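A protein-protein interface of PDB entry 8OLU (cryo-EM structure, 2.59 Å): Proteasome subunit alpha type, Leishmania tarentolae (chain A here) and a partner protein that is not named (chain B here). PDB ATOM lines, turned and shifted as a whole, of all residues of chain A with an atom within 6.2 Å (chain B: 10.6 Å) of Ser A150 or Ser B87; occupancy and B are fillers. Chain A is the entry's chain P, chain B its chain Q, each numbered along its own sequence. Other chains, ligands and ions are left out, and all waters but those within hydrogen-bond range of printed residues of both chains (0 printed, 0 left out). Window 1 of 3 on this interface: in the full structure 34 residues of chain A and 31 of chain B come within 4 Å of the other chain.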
ATOM      1  N   ILE A  20      -2.403  -0.569 -16.399  1.00  0.00           N
ATOM      2  CA  ILE A  20      -3.766  -0.247 -16.013  1.00  0.00           C
ATOM      3  C   ILE A  20      -4.393  -1.312 -15.174  1.00  0.00           C
ATOM      4  O   ILE A  20      -5.212  -0.937 -14.366  1.00  0.00           O
ATOM      5  CB  ILE A  20      -4.663   0.017 -17.213  1.00  0.00           C
ATOM      6  CG1 ILE A  20      -4.261   1.296 -17.906  1.00  0.00           C
ATOM      7  CG2 ILE A  20      -6.114   0.113 -16.844  1.00  0.00           C
ATOM      8  CD1 ILE A  20      -4.961   1.412 -19.261  1.00  0.00           C
ATOM      9  N   THR A  24      -5.575  -0.713 -11.415  1.00  0.00           N
ATOM     10  CA  THR A  24      -6.889  -1.160 -11.001  1.00  0.00           C
ATOM     11  C   THR A  24      -6.791  -1.983  -9.741  1.00  0.00           C
ATOM     12  O   THR A  24      -7.677  -1.930  -8.911  1.00  0.00           O
ATOM     13  CB  THR A  24      -7.601  -1.880 -12.139  1.00  0.00           C
ATOM     14  OG1 THR A  24      -7.899  -0.969 -13.207  1.00  0.00           O
ATOM     15  CG2 THR A  24      -8.912  -2.438 -11.649  1.00  0.00           C
ATOM     16  N   SER A 113     -13.439  10.626 -16.862  1.00  0.00           N
ATOM     17  CA  SER A 113     -13.044   9.487 -17.640  1.00  0.00           C
ATOM     18  C   SER A 113     -11.923   9.864 -18.560  1.00  0.00           C
ATOM     19  O   SER A 113     -11.080   9.063 -18.838  1.00  0.00           O
ATOM     20  CB  SER A 113     -14.255   9.017 -18.426  1.00  0.00           C
ATOM     21  OG  SER A 113     -13.868   8.141 -19.450  1.00  0.00           O
ATOM     22  N   TYR A 116      -8.644  10.312 -16.719  1.00  0.00           N
ATOM     23  CA  TYR A 116      -8.061   9.025 -16.539  1.00  0.00           C
ATOM     24  C   TYR A 116      -7.465   8.467 -17.814  1.00  0.00           C
ATOM     25  O   TYR A 116      -6.366   7.912 -17.793  1.00  0.00           O
ATOM     26  CB  TYR A 116      -9.099   8.036 -16.135  1.00  0.00           C
ATOM     27  CG  TYR A 116      -9.434   7.997 -14.678  1.00  0.00           C
ATOM     28  CD1 TYR A 116      -8.634   7.332 -13.778  1.00  0.00           C
ATOM     29  CD2 TYR A 116     -10.639   8.428 -14.220  1.00  0.00           C
ATOM     30  CE1 TYR A 116      -8.971   7.153 -12.451  1.00  0.00           C
ATOM     31  CE2 TYR A 116     -11.018   8.216 -12.906  1.00  0.00           C
ATOM     32  CZ  TYR A 116     -10.212   7.555 -12.011  1.00  0.00           C
ATOM     33  OH  TYR A 116     -10.629   7.381 -10.701  1.00  0.00           O
ATOM     34  N   GLN A 117      -8.181   8.536 -18.916  1.00  0.00           N
ATOM     35  CA  GLN A 117      -7.627   7.995 -20.143  1.00  0.00           C
ATOM     36  C   GLN A 117      -6.332   8.685 -20.507  1.00  0.00           C
ATOM     37  O   GLN A 117      -5.416   7.987 -20.888  1.00  0.00           O
ATOM     38  CB  GLN A 117      -8.594   8.170 -21.292  1.00  0.00           C
ATOM     39  CG  GLN A 117      -8.241   7.392 -22.546  1.00  0.00           C
ATOM     40  CD  GLN A 117      -7.300   8.060 -23.518  1.00  0.00           C
ATOM     41  OE1 GLN A 117      -7.274   9.282 -23.662  1.00  0.00           O
ATOM     42  NE2 GLN A 117      -6.516   7.215 -24.184  1.00  0.00           N
ATOM     43  N   THR A 120      -3.355   7.120 -19.285  1.00  0.00           N
ATOM     44  CA  THR A 120      -3.101   5.754 -19.722  1.00  0.00           C
ATOM     45  C   THR A 120      -2.364   5.751 -21.057  1.00  0.00           C
ATOM     46  O   THR A 120      -2.162   4.704 -21.650  1.00  0.00           O
ATOM     47  CB  THR A 120      -4.416   4.985 -19.933  1.00  0.00           C
ATOM     48  OG1 THR A 120      -5.174   5.522 -21.020  1.00  0.00           O
ATOM     49  CG2 THR A 120      -5.313   5.017 -18.723  1.00  0.00           C
ATOM     50  N   PHE A 128      -3.836   6.569 -12.846  1.00  0.00           N
ATOM     51  CA  PHE A 128      -4.333   6.891 -11.531  1.00  0.00           C
ATOM     52  C   PHE A 128      -4.684   5.618 -10.856  1.00  0.00           C
ATOM     53  O   PHE A 128      -5.192   4.720 -11.512  1.00  0.00           O
ATOM     54  CB  PHE A 128      -5.593   7.701 -11.628  1.00  0.00           C
ATOM     55  CG  PHE A 128      -5.279   9.105 -12.040  1.00  0.00           C
ATOM     56  CD1 PHE A 128      -4.648   9.955 -11.185  1.00  0.00           C
ATOM     57  CD2 PHE A 128      -5.618   9.568 -13.288  1.00  0.00           C
ATOM     58  CE1 PHE A 128      -4.466  11.277 -11.528  1.00  0.00           C
ATOM     59  CE2 PHE A 128      -5.383  10.880 -13.678  1.00  0.00           C
ATOM     60  CZ  PHE A 128      -4.787  11.725 -12.795  1.00  0.00           C
ATOM     61  N   ASP A 148     -13.287   3.943 -13.192  1.00  0.00           N
ATOM     62  CA  ASP A 148     -12.117   3.170 -12.875  1.00  0.00           C
ATOM     63  C   ASP A 148     -10.925   3.832 -13.523  1.00  0.00           C
ATOM     64  O   ASP A 148     -11.068   4.827 -14.237  1.00  0.00           O
ATOM     65  CB  ASP A 148     -12.290   1.726 -13.310  1.00  0.00           C
ATOM     66  CG  ASP A 148     -13.181   0.939 -12.341  1.00  0.00           C
ATOM     67  OD1 ASP A 148     -13.511   1.492 -11.221  1.00  0.00           O
ATOM     68  OD2 ASP A 148     -13.553  -0.233 -12.680  1.00  0.00           O
ATOM     69  N   PRO A 149      -9.707   3.410 -13.167  1.00  0.00           N
ATOM     70  CA  PRO A 149      -8.496   3.918 -13.796  1.00  0.00           C
ATOM     71  C   PRO A 149      -8.300   3.685 -15.288  1.00  0.00           C
ATOM     72  O   PRO A 149      -7.323   4.147 -15.862  1.00  0.00           O
ATOM     73  CB  PRO A 149      -7.416   3.034 -13.148  1.00  0.00           C
ATOM     74  CG  PRO A 149      -7.968   2.749 -11.824  1.00  0.00           C
ATOM     75  CD  PRO A 149      -9.438   2.501 -12.067  1.00  0.00           C
ATOM     76  N   SER A 150      -9.071   2.772 -15.866  1.00  0.00           N
ATOM     77  CA  SER A 150      -9.015   2.575 -17.302  1.00  0.00           C
ATOM     78  C   SER A 150      -9.628   3.809 -17.938  1.00  0.00           C
ATOM     79  O   SER A 150      -9.408   4.117 -19.092  1.00  0.00           O
ATOM     80  CB  SER A 150      -9.772   1.347 -17.675  1.00  0.00           C
ATOM     81  OG  SER A 150     -11.110   1.450 -17.210  1.00  0.00           O
ATOM     82  N   GLY A 151     -10.395   4.519 -17.130  1.00  0.00           N
ATOM     83  CA  GLY A 151     -11.200   5.635 -17.594  1.00  0.00           C
ATOM     84  C   GLY A 151     -12.614   5.231 -17.960  1.00  0.00           C
ATOM     85  O   GLY A 151     -13.379   6.053 -18.421  1.00  0.00           O
ATOM     86  N   THR A 152     -12.892   3.956 -17.748  1.00  0.00           N
ATOM     87  CA  THR A 152     -14.176   3.382 -18.005  1.00  0.00           C
ATOM     88  C   THR A 152     -15.135   3.837 -16.935  1.00  0.00           C
ATOM     89  O   THR A 152     -14.752   4.078 -15.814  1.00  0.00           O
ATOM     90  CB  THR A 152     -14.078   1.866 -17.979  1.00  0.00           C
ATOM     91  OG1 THR A 152     -13.361   1.423 -19.129  1.00  0.00           O
ATOM     92  CG2 THR A 152     -15.426   1.200 -18.042  1.00  0.00           C
ATOM     93  N   PHE A 153     -16.401   3.926 -17.266  1.00  0.00           N
ATOM     94  CA  PHE A 153     -17.314   4.238 -16.224  1.00  0.00           C
ATOM     95  C   PHE A 153     -18.633   3.585 -16.486  1.00  0.00           C
ATOM     96  O   PHE A 153     -18.975   3.396 -17.616  1.00  0.00           O
ATOM     97  CB  PHE A 153     -17.471   5.750 -16.188  1.00  0.00           C
ATOM     98  CG  PHE A 153     -18.023   6.384 -17.418  1.00  0.00           C
ATOM     99  CD1 PHE A 153     -19.371   6.398 -17.651  1.00  0.00           C
ATOM    100  CD2 PHE A 153     -17.175   6.822 -18.402  1.00  0.00           C
ATOM    101  CE1 PHE A 153     -19.880   6.938 -18.816  1.00  0.00           C
ATOM    102  CE2 PHE A 153     -17.685   7.364 -19.585  1.00  0.00           C
ATOM    103  CZ  PHE A 153     -19.043   7.439 -19.788  1.00  0.00           C
ATOM    104  N   ALA B  31     -12.539  -8.006 -27.391  1.00  0.00           N
ATOM    105  CA  ALA B  31     -13.714  -7.172 -27.186  1.00  0.00           C
ATOM    106  C   ALA B  31     -15.023  -7.757 -27.718  1.00  0.00           C
ATOM    107  O   ALA B  31     -15.073  -8.565 -28.638  1.00  0.00           O
ATOM    108  CB  ALA B  31     -13.474  -5.856 -27.861  1.00  0.00           C
ATOM    109  N   GLU B  69     -24.198   1.416 -25.579  1.00  0.00           N
ATOM    110  CA  GLU B  69     -23.077   0.792 -24.938  1.00  0.00           C
ATOM    111  C   GLU B  69     -22.015   0.511 -26.008  1.00  0.00           C
ATOM    112  O   GLU B  69     -20.806   0.659 -25.793  1.00  0.00           O
ATOM    113  CB  GLU B  69     -23.677  -0.406 -24.203  1.00  0.00           C
ATOM    114  CG  GLU B  69     -22.763  -1.012 -23.144  1.00  0.00           C
ATOM    115  CD  GLU B  69     -23.297  -2.305 -22.542  1.00  0.00           C
ATOM    116  OE1 GLU B  69     -22.589  -3.341 -22.682  1.00  0.00           O
ATOM    117  OE2 GLU B  69     -24.427  -2.267 -21.947  1.00  0.00           O
ATOM    118  N   LYS B  70     -22.473   0.136 -27.199  1.00  0.00           N
ATOM    119  CA  LYS B  70     -21.558  -0.171 -28.275  1.00  0.00           C
ATOM    120  C   LYS B  70     -21.619   0.903 -29.370  1.00  0.00           C
ATOM    121  O   LYS B  70     -20.607   1.127 -30.007  1.00  0.00           O
ATOM    122  CB  LYS B  70     -21.859  -1.603 -28.744  1.00  0.00           C
ATOM    123  CG  LYS B  70     -21.537  -2.705 -27.733  1.00  0.00           C
ATOM    124  CD  LYS B  70     -20.036  -2.944 -27.464  1.00  0.00           C
ATOM    125  CE  LYS B  70     -19.392  -3.778 -28.559  1.00  0.00           C
ATOM    126  NZ  LYS B  70     -17.900  -3.773 -28.567  1.00  0.00           N
ATOM    127  N   TYR B  72     -22.360   4.690 -31.217  1.00  0.00           N
ATOM    128  CA  TYR B  72     -22.354   6.111 -30.964  1.00  0.00           C
ATOM    129  C   TYR B  72     -22.626   6.878 -32.230  1.00  0.00           C
ATOM    130  O   TYR B  72     -22.140   6.545 -33.294  1.00  0.00           O
ATOM    131  CB  TYR B  72     -20.976   6.538 -30.503  1.00  0.00           C
ATOM    132  CG  TYR B  72     -20.505   5.756 -29.316  1.00  0.00           C
ATOM    133  CD1 TYR B  72     -20.873   6.091 -28.030  1.00  0.00           C
ATOM    134  CD2 TYR B  72     -19.726   4.644 -29.493  1.00  0.00           C
ATOM    135  CE1 TYR B  72     -20.486   5.313 -26.953  1.00  0.00           C
ATOM    136  CE2 TYR B  72     -19.298   3.879 -28.427  1.00  0.00           C
ATOM    137  CZ  TYR B  72     -19.693   4.196 -27.146  1.00  0.00           C
ATOM    138  OH  TYR B  72     -19.216   3.410 -26.109  1.00  0.00           O
ATOM    139  N   VAL B  82     -17.597   0.412 -31.673  1.00  0.00           N
ATOM    140  CA  VAL B  82     -16.195   0.282 -31.408  1.00  0.00           C
ATOM    141  C   VAL B  82     -16.021  -1.061 -30.776  1.00  0.00           C
ATOM    142  O   VAL B  82     -16.916  -1.553 -30.109  1.00  0.00           O
ATOM    143  CB  VAL B  82     -15.688   1.368 -30.467  1.00  0.00           C
ATOM    144  CG1 VAL B  82     -16.031   2.749 -30.994  1.00  0.00           C
ATOM    145  CG2 VAL B  82     -16.269   1.201 -29.071  1.00  0.00           C
ATOM    146  N   ALA B  83     -14.826  -1.547 -30.962  1.00  0.00           N
ATOM    147  CA  ALA B  83     -14.347  -2.670 -30.220  1.00  0.00           C
ATOM    148  C   ALA B  83     -12.979  -2.291 -29.699  1.00  0.00           C
ATOM    149  O   ALA B  83     -12.185  -1.688 -30.426  1.00  0.00           O
ATOM    150  CB  ALA B  83     -14.262  -3.818 -31.158  1.00  0.00           C
ATOM    151  N   GLY B  84     -12.711  -2.627 -28.446  1.00  0.00           N
ATOM    152  CA  GLY B  84     -11.358  -2.502 -27.925  1.00  0.00           C
ATOM    153  C   GLY B  84     -11.420  -1.605 -26.713  1.00  0.00           C
ATOM    154  O   GLY B  84     -12.493  -1.409 -26.147  1.00  0.00           O
ATOM    155  N   VAL B  85     -10.317  -0.966 -26.411  1.00  0.00           N
ATOM    156  CA  VAL B  85     -10.182  -0.237 -25.173  1.00  0.00           C
ATOM    157  C   VAL B  85     -11.209   0.881 -25.177  1.00  0.00           C
ATOM    158  O   VAL B  85     -11.073   1.849 -25.884  1.00  0.00           O
ATOM    159  CB  VAL B  85      -8.728   0.261 -25.075  1.00  0.00           C
ATOM    160  CG1 VAL B  85      -8.456   1.169 -23.877  1.00  0.00           C
ATOM    161  CG2 VAL B  85      -7.764  -0.913 -25.138  1.00  0.00           C
ATOM    162  N   THR B  86     -12.250   0.715 -24.387  1.00  0.00           N
ATOM    163  CA  THR B  86     -13.387   1.611 -24.438  1.00  0.00           C
ATOM    164  C   THR B  86     -12.980   3.068 -24.280  1.00  0.00           C
ATOM    165  O   THR B  86     -13.501   3.929 -24.963  1.00  0.00           O
ATOM    166  CB  THR B  86     -14.362   1.333 -23.295  1.00  0.00           C
ATOM    167  OG1 THR B  86     -14.695  -0.060 -23.366  1.00  0.00           O
ATOM    168  CG2 THR B  86     -15.568   2.252 -23.349  1.00  0.00           C
ATOM    169  N   SER B  87     -12.073   3.357 -23.365  1.00  0.00           N
ATOM    170  CA  SER B  87     -11.760   4.747 -23.080  1.00  0.00           C
ATOM    171  C   SER B  87     -11.040   5.406 -24.233  1.00  0.00           C
ATOM    172  O   SER B  87     -11.165   6.618 -24.388  1.00  0.00           O
ATOM    173  CB  SER B  87     -10.923   4.864 -21.848  1.00  0.00           C
ATOM    174  OG  SER B  87     -11.782   4.904 -20.716  1.00  0.00           O
ATOM    175  N   ASP B  88     -10.212   4.626 -24.948  1.00  0.00           N
ATOM    176  CA  ASP B  88      -9.575   5.095 -26.167  1.00  0.00           C
ATOM    177  C   ASP B  88     -10.648   5.482 -27.171  1.00  0.00           C
ATOM    178  O   ASP B  88     -10.621   6.582 -27.723  1.00  0.00           O
ATOM    179  CB  ASP B  88      -8.588   4.058 -26.692  1.00  0.00           C
ATOM    180  CG  ASP B  88      -7.268   3.965 -25.890  1.00  0.00           C
ATOM    181  OD1 ASP B  88      -7.060   4.818 -24.931  1.00  0.00           O
ATOM    182  OD2 ASP B  88      -6.422   3.060 -26.201  1.00  0.00           O
ATOM    183  N   ALA B  89     -11.656   4.633 -27.294  1.00  0.00           N
ATOM    184  CA  ALA B  89     -12.792   4.916 -28.128  1.00  0.00           C
ATOM    185  C   ALA B  89     -13.325   6.294 -27.835  1.00  0.00           C
ATOM    186  O   ALA B  89     -13.458   7.065 -28.757  1.00  0.00           O
ATOM    187  CB  ALA B  89     -13.866   3.912 -27.910  1.00  0.00           C
ATOM    188  N   TYR B  90     -13.652   6.592 -26.587  1.00  0.00           N
ATOM    189  CA  TYR B  90     -14.219   7.894 -26.315  1.00  0.00           C
ATOM    190  C   TYR B  90     -13.275   9.049 -26.690  1.00  0.00           C
ATOM    191  O   TYR B  90     -13.722  10.090 -27.158  1.00  0.00           O
ATOM    192  CB  TYR B  90     -14.650   7.997 -24.864  1.00  0.00           C
ATOM    193  CG  TYR B  90     -15.924   7.271 -24.533  1.00  0.00           C
ATOM    194  CD1 TYR B  90     -17.161   7.856 -24.770  1.00  0.00           C
ATOM    195  CD2 TYR B  90     -15.899   6.065 -23.862  1.00  0.00           C
ATOM    196  CE1 TYR B  90     -18.343   7.228 -24.401  1.00  0.00           C
ATOM    197  CE2 TYR B  90     -17.068   5.408 -23.513  1.00  0.00           C
ATOM    198  CZ  TYR B  90     -18.296   5.983 -23.786  1.00  0.00           C
ATOM    199  OH  TYR B  90     -19.448   5.314 -23.405  1.00  0.00           O
ATOM    200  N   ALA B  91     -11.967   8.885 -26.542  1.00  0.00           N
ATOM    201  CA  ALA B  91     -11.076   9.944 -26.983  1.00  0.00           C
ATOM    202  C   ALA B  91     -11.257  10.204 -28.476  1.00  0.00           C
ATOM    203  O   ALA B  91     -11.457  11.349 -28.867  1.00  0.00           O
ATOM    204  CB  ALA B  91      -9.643   9.643 -26.659  1.00  0.00           C
ATOM    205  N   LEU B  92     -11.188   9.136 -29.268  1.00  0.00           N
ATOM    206  CA  LEU B  92     -11.352   9.204 -30.705  1.00  0.00           C
ATOM    207  C   LEU B  92     -12.747   9.648 -31.130  1.00  0.00           C
ATOM    208  O   LEU B  92     -12.912  10.424 -32.049  1.00  0.00           O
ATOM    209  CB  LEU B  92     -11.101   7.806 -31.255  1.00  0.00           C
ATOM    210  CG  LEU B  92      -9.635   7.418 -31.273  1.00  0.00           C
ATOM    211  CD1 LEU B  92      -9.497   5.998 -31.771  1.00  0.00           C
ATOM    212  CD2 LEU B  92      -8.834   8.387 -32.131  1.00  0.00           C
ATOM    213  N   LEU B  93     -13.759   9.042 -30.564  1.00  0.00           N
ATOM    214  CA  LEU B  93     -15.106   9.440 -30.848  1.00  0.00           C
ATOM    215  C   LEU B  93     -15.272  10.939 -30.706  1.00  0.00           C
ATOM    216  O   LEU B  93     -16.063  11.562 -31.407  1.00  0.00           O
ATOM    217  CB  LEU B  93     -16.025   8.746 -29.855  1.00  0.00           C
ATOM    218  CG  LEU B  93     -17.472   9.195 -29.986  1.00  0.00           C
ATOM    219  CD1 LEU B  93     -18.073   8.491 -31.180  1.00  0.00           C
ATOM    220  CD2 LEU B  93     -18.284   8.923 -28.728  1.00  0.00           C
ATOM    221  N   ASN B  94     -14.635  11.535 -29.720  1.00  0.00           N
ATOM    222  CA  ASN B  94     -14.833  12.956 -29.530  1.00  0.00           C
ATOM    223  C   ASN B  94     -14.108  13.650 -30.663  1.00  0.00           C
ATOM    224  O   ASN B  94     -14.604  14.627 -31.221  1.00  0.00           O
ATOM    225  CB  ASN B  94     -14.355  13.415 -28.156  1.00  0.00           C
ATOM    226  CG  ASN B  94     -14.450  14.921 -27.991  1.00  0.00           C
ATOM    227  OD1 ASN B  94     -15.539  15.417 -27.714  1.00  0.00           O
ATOM    228  ND2 ASN B  94     -13.348  15.648 -28.197  1.00  0.00           N
ATOM    229  N   TYR B  95     -12.922  13.151 -31.007  1.00  0.00           N
ATOM    230  CA  TYR B  95     -12.215  13.669 -32.156  1.00  0.00           C
ATOM    231  C   TYR B  95     -13.020  13.539 -33.454  1.00  0.00           C
ATOM    232  O   TYR B  95     -13.082  14.441 -34.275  1.00  0.00           O
ATOM    233  CB  TYR B  95     -10.918  12.909 -32.308  1.00  0.00           C
ATOM    234  CG  TYR B  95     -10.013  13.446 -33.373  1.00  0.00           C
ATOM    235  CD1 TYR B  95      -9.431  14.690 -33.265  1.00  0.00           C
ATOM    236  CD2 TYR B  95      -9.745  12.710 -34.503  1.00  0.00           C
ATOM    237  CE1 TYR B  95      -8.581  15.189 -34.249  1.00  0.00           C
ATOM    238  CE2 TYR B  95      -8.884  13.182 -35.482  1.00  0.00           C
ATOM    239  CZ  TYR B  95      -8.277  14.419 -35.353  1.00  0.00           C
ATOM    240  OH  TYR B  95      -7.428  14.839 -36.342  1.00  0.00           O
ATOM    241  N   ARG B 134       1.697   4.684 -26.587  1.00  0.00           N
ATOM    242  CA  ARG B 134       1.132   3.440 -27.144  1.00  0.00           C
ATOM    243  C   ARG B 134       0.067   3.846 -28.126  1.00  0.00           C
ATOM    244  O   ARG B 134      -0.351   4.979 -28.073  1.00  0.00           O
ATOM    245  CB  ARG B 134       0.446   2.528 -26.124  1.00  0.00           C
ATOM    246  CG  ARG B 134      -0.721   3.206 -25.450  1.00  0.00           C
ATOM    247  CD  ARG B 134      -1.446   2.345 -24.454  1.00  0.00           C
ATOM    248  NE  ARG B 134      -2.529   3.142 -23.889  1.00  0.00           N
ATOM    249  CZ  ARG B 134      -3.787   3.145 -24.334  1.00  0.00           C
ATOM    250  NH1 ARG B 134      -4.143   2.557 -25.469  1.00  0.00           N
ATOM    251  NH2 ARG B 134      -4.673   3.835 -23.644  1.00  0.00           N
ATOM    252  N   PRO B 135      -0.350   3.006 -29.075  1.00  0.00           N
ATOM    253  CA  PRO B 135      -1.443   3.344 -29.948  1.00  0.00           C
ATOM    254  C   PRO B 135      -2.812   3.299 -29.298  1.00  0.00           C
ATOM    255  O   PRO B 135      -2.977   2.811 -28.184  1.00  0.00           O
ATOM    256  CB  PRO B 135      -1.384   2.288 -31.041  1.00  0.00           C
ATOM    257  CG  PRO B 135      -0.629   1.200 -30.491  1.00  0.00           C
ATOM    258  CD  PRO B 135       0.308   1.783 -29.491  1.00  0.00           C
ATOM    259  N   TYR B 136      -3.795   3.862 -29.986  1.00  0.00           N
ATOM    260  CA  TYR B 136      -5.173   3.693 -29.576  1.00  0.00           C
ATOM    261  C   TYR B 136      -5.532   2.266 -29.872  1.00  0.00           C
ATOM    262  O   TYR B 136      -5.244   1.790 -30.960  1.00  0.00           O
ATOM    263  CB  TYR B 136      -6.090   4.585 -30.383  1.00  0.00           C
ATOM    264  CG  TYR B 136      -5.950   6.034 -30.062  1.00  0.00           C
ATOM    265  CD1 TYR B 136      -6.577   6.567 -28.950  1.00  0.00           C
ATOM    266  CD2 TYR B 136      -5.192   6.866 -30.843  1.00  0.00           C
ATOM    267  CE1 TYR B 136      -6.520   7.923 -28.641  1.00  0.00           C
ATOM    268  CE2 TYR B 136      -5.118   8.226 -30.562  1.00  0.00           C
ATOM    269  CZ  TYR B 136      -5.790   8.760 -29.459  1.00  0.00           C
ATOM    270  OH  TYR B 136      -5.743  10.098 -29.142  1.00  0.00           O
ATOM    271  N   GLY B 137      -6.131   1.614 -28.897  1.00  0.00           N
ATOM    272  CA  GLY B 137      -6.387   0.205 -29.014  1.00  0.00           C
ATOM    273  C   GLY B 137      -7.829   0.005 -29.361  1.00  0.00           C
ATOM    274  O   GLY B 137      -8.539  -0.559 -28.578  1.00  0.00           O
ATOM    275  N   VAL B 138      -8.205   0.459 -30.548  1.00  0.00           N
ATOM    276  CA  VAL B 138      -9.598   0.610 -30.931  1.00  0.00           C
ATOM    277  C   VAL B 138      -9.796   0.287 -32.399  1.00  0.00           C
ATOM    278  O   VAL B 138      -8.908   0.432 -33.205  1.00  0.00           O
ATOM    279  CB  VAL B 138      -9.992   2.057 -30.666  1.00  0.00           C
ATOM    280  CG1 VAL B 138     -11.141   2.516 -31.503  1.00  0.00           C
ATOM    281  CG2 VAL B 138     -10.369   2.223 -29.234  1.00  0.00           C
ATOM    282  N   SER B 139     -10.953  -0.238 -32.717  1.00  0.00           N
ATOM    283  CA  SER B 139     -11.357  -0.493 -34.080  1.00  0.00           C
ATOM    284  C   SER B 139     -12.749   0.058 -34.176  1.00  0.00           C
ATOM    285  O   SER B 139     -13.610  -0.404 -33.446  1.00  0.00           O
ATOM    286  CB  SER B 139     -11.431  -1.953 -34.452  1.00  0.00           C
ATOM    287  OG  SER B 139     -10.481  -2.289 -35.429  1.00  0.00           O
ATOM    288  N   PHE B 140     -12.957   0.944 -35.138  1.00  0.00           N
ATOM    289  CA  PHE B 140     -14.309   1.328 -35.429  1.00  0.00           C
ATOM    290  C   PHE B 140     -14.923   0.475 -36.510  1.00  0.00           C
ATOM    291  O   PHE B 140     -14.220  -0.040 -37.350  1.00  0.00           O
ATOM    292  CB  PHE B 140     -14.317   2.768 -35.861  1.00  0.00           C
ATOM    293  CG  PHE B 140     -13.994   3.658 -34.718  1.00  0.00           C
ATOM    294  CD1 PHE B 140     -15.002   4.175 -33.937  1.00  0.00           C
ATOM    295  CD2 PHE B 140     -12.684   3.957 -34.426  1.00  0.00           C
ATOM    296  CE1 PHE B 140     -14.711   5.002 -32.866  1.00  0.00           C
ATOM    297  CE2 PHE B 140     -12.393   4.818 -33.376  1.00  0.00           C
ATOM    298  CZ  PHE B 140     -13.406   5.330 -32.593  1.00  0.00           C
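Of the 13 printed residues of chain A, 5 touch a printed residue of chain B.
Of the 25 printed residues of chain B, 4 touch a printed residue of chain A.
Printed residues of chain B that touch a printed residue of chain A: Ser B87, Asp B88, Ala B91 and Arg B134.
Hydrophobic or aromatic side chains of chain B within 4 Å of the printed part of chain A: Ala B91.
Among the printed residues, 8 pairs touch across the chains.
Among the printed residues, no Asp or Glu carboxylate lies within 4 Å of a Lys or Arg side-chain nitrogen of the other chain.
The backbone carbonyl oxygen (O) of Thr A120 lies within hydrogen-bond range of the guanidinium group (NE) of Arg B134, 2.8 Å away.
The side-chain carboxylate (OD1) of Asp B88 is in hydrogen-bond range of the side-chain amide nitrogen (NE2) of Gln A117 (2.6 Å).
The side-chain hydroxyl (OG) of Ser B87 is in hydrogen-bond range of the backbone NH (N) of Thr A152, at 3.3 Å.
OG of Ser B87 is in hydrogen-bond range of O of Ser A150.
The side-chain hydroxyl (OG) of Ser B87 sits close to the backbone carbonyl oxygen (O) of Gly A151 (3.0 Å).
The side-chain carboxylate (OD2) of Asp B88 sits at hydrogen-bond distance from the backbone NH (N) of Gly B137 (3.1 Å).
O of Gln A117 sits at hydrogen-bond distance from OG1 of Thr A120 (2.5 Å).
The side-chain hydroxyl (OG) of Ser A150 is in hydrogen-bond range of the side-chain hydroxyl (OG1) of Thr A152, 3.0 Å away.
The side-chain carboxylate (OD2) of Asp B88 lies within salt-bridge range of the guanidinium group (NH1) of Arg B134 (2.4 Å).
Printed residues of chain B within 4 Å of Gln A117: Ser B87, Asp B88, Ala B91 and Arg B134.
Printed residues of chain B within 4 Å of Thr A120: Arg B134 (2.8 Å).
No residue of chain B comes within 4 Å of Asp A148.
No residue of chain B comes within 4 Å of Pro A149.
Ser A150 touches just one residue of chain B: Ser B87.
Of the printed residues of chain B, Gly A151 touches Ser B87 (2.9 Å).
Of chain B, only Ser B87 (3.3 Å) comes within 4 Å of Thr A152.
Printed residues of chain A within 4 Å of Ser B87: Gln A117, Ser A150, Gly A151 and Thr A152.
Printed residues of chain A within 4 Å of Asp B88: Gln A117 (2.6 Å).
Of the printed residues of chain A, Ala B91 touches Gln A117.
Of the printed residues of chain A, Arg B134 touches Gln A117 (3.9 Å) and Thr A120 (2.8 Å).
The nearest residue of chain B that does not touch Ser A150 is Val B85 (5.7 Å).
The nearest printed residue of chain A that does not touch Ala B91 is Ser A113 (7.4 Å).
Among the printed residues, pairs that only touch across the chains: Gln A117 with Ser B87 (3.5 Å), Gln A117 with Ala B91 (3.8 Å) and Gln A117 with Arg B134 (3.9 Å).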
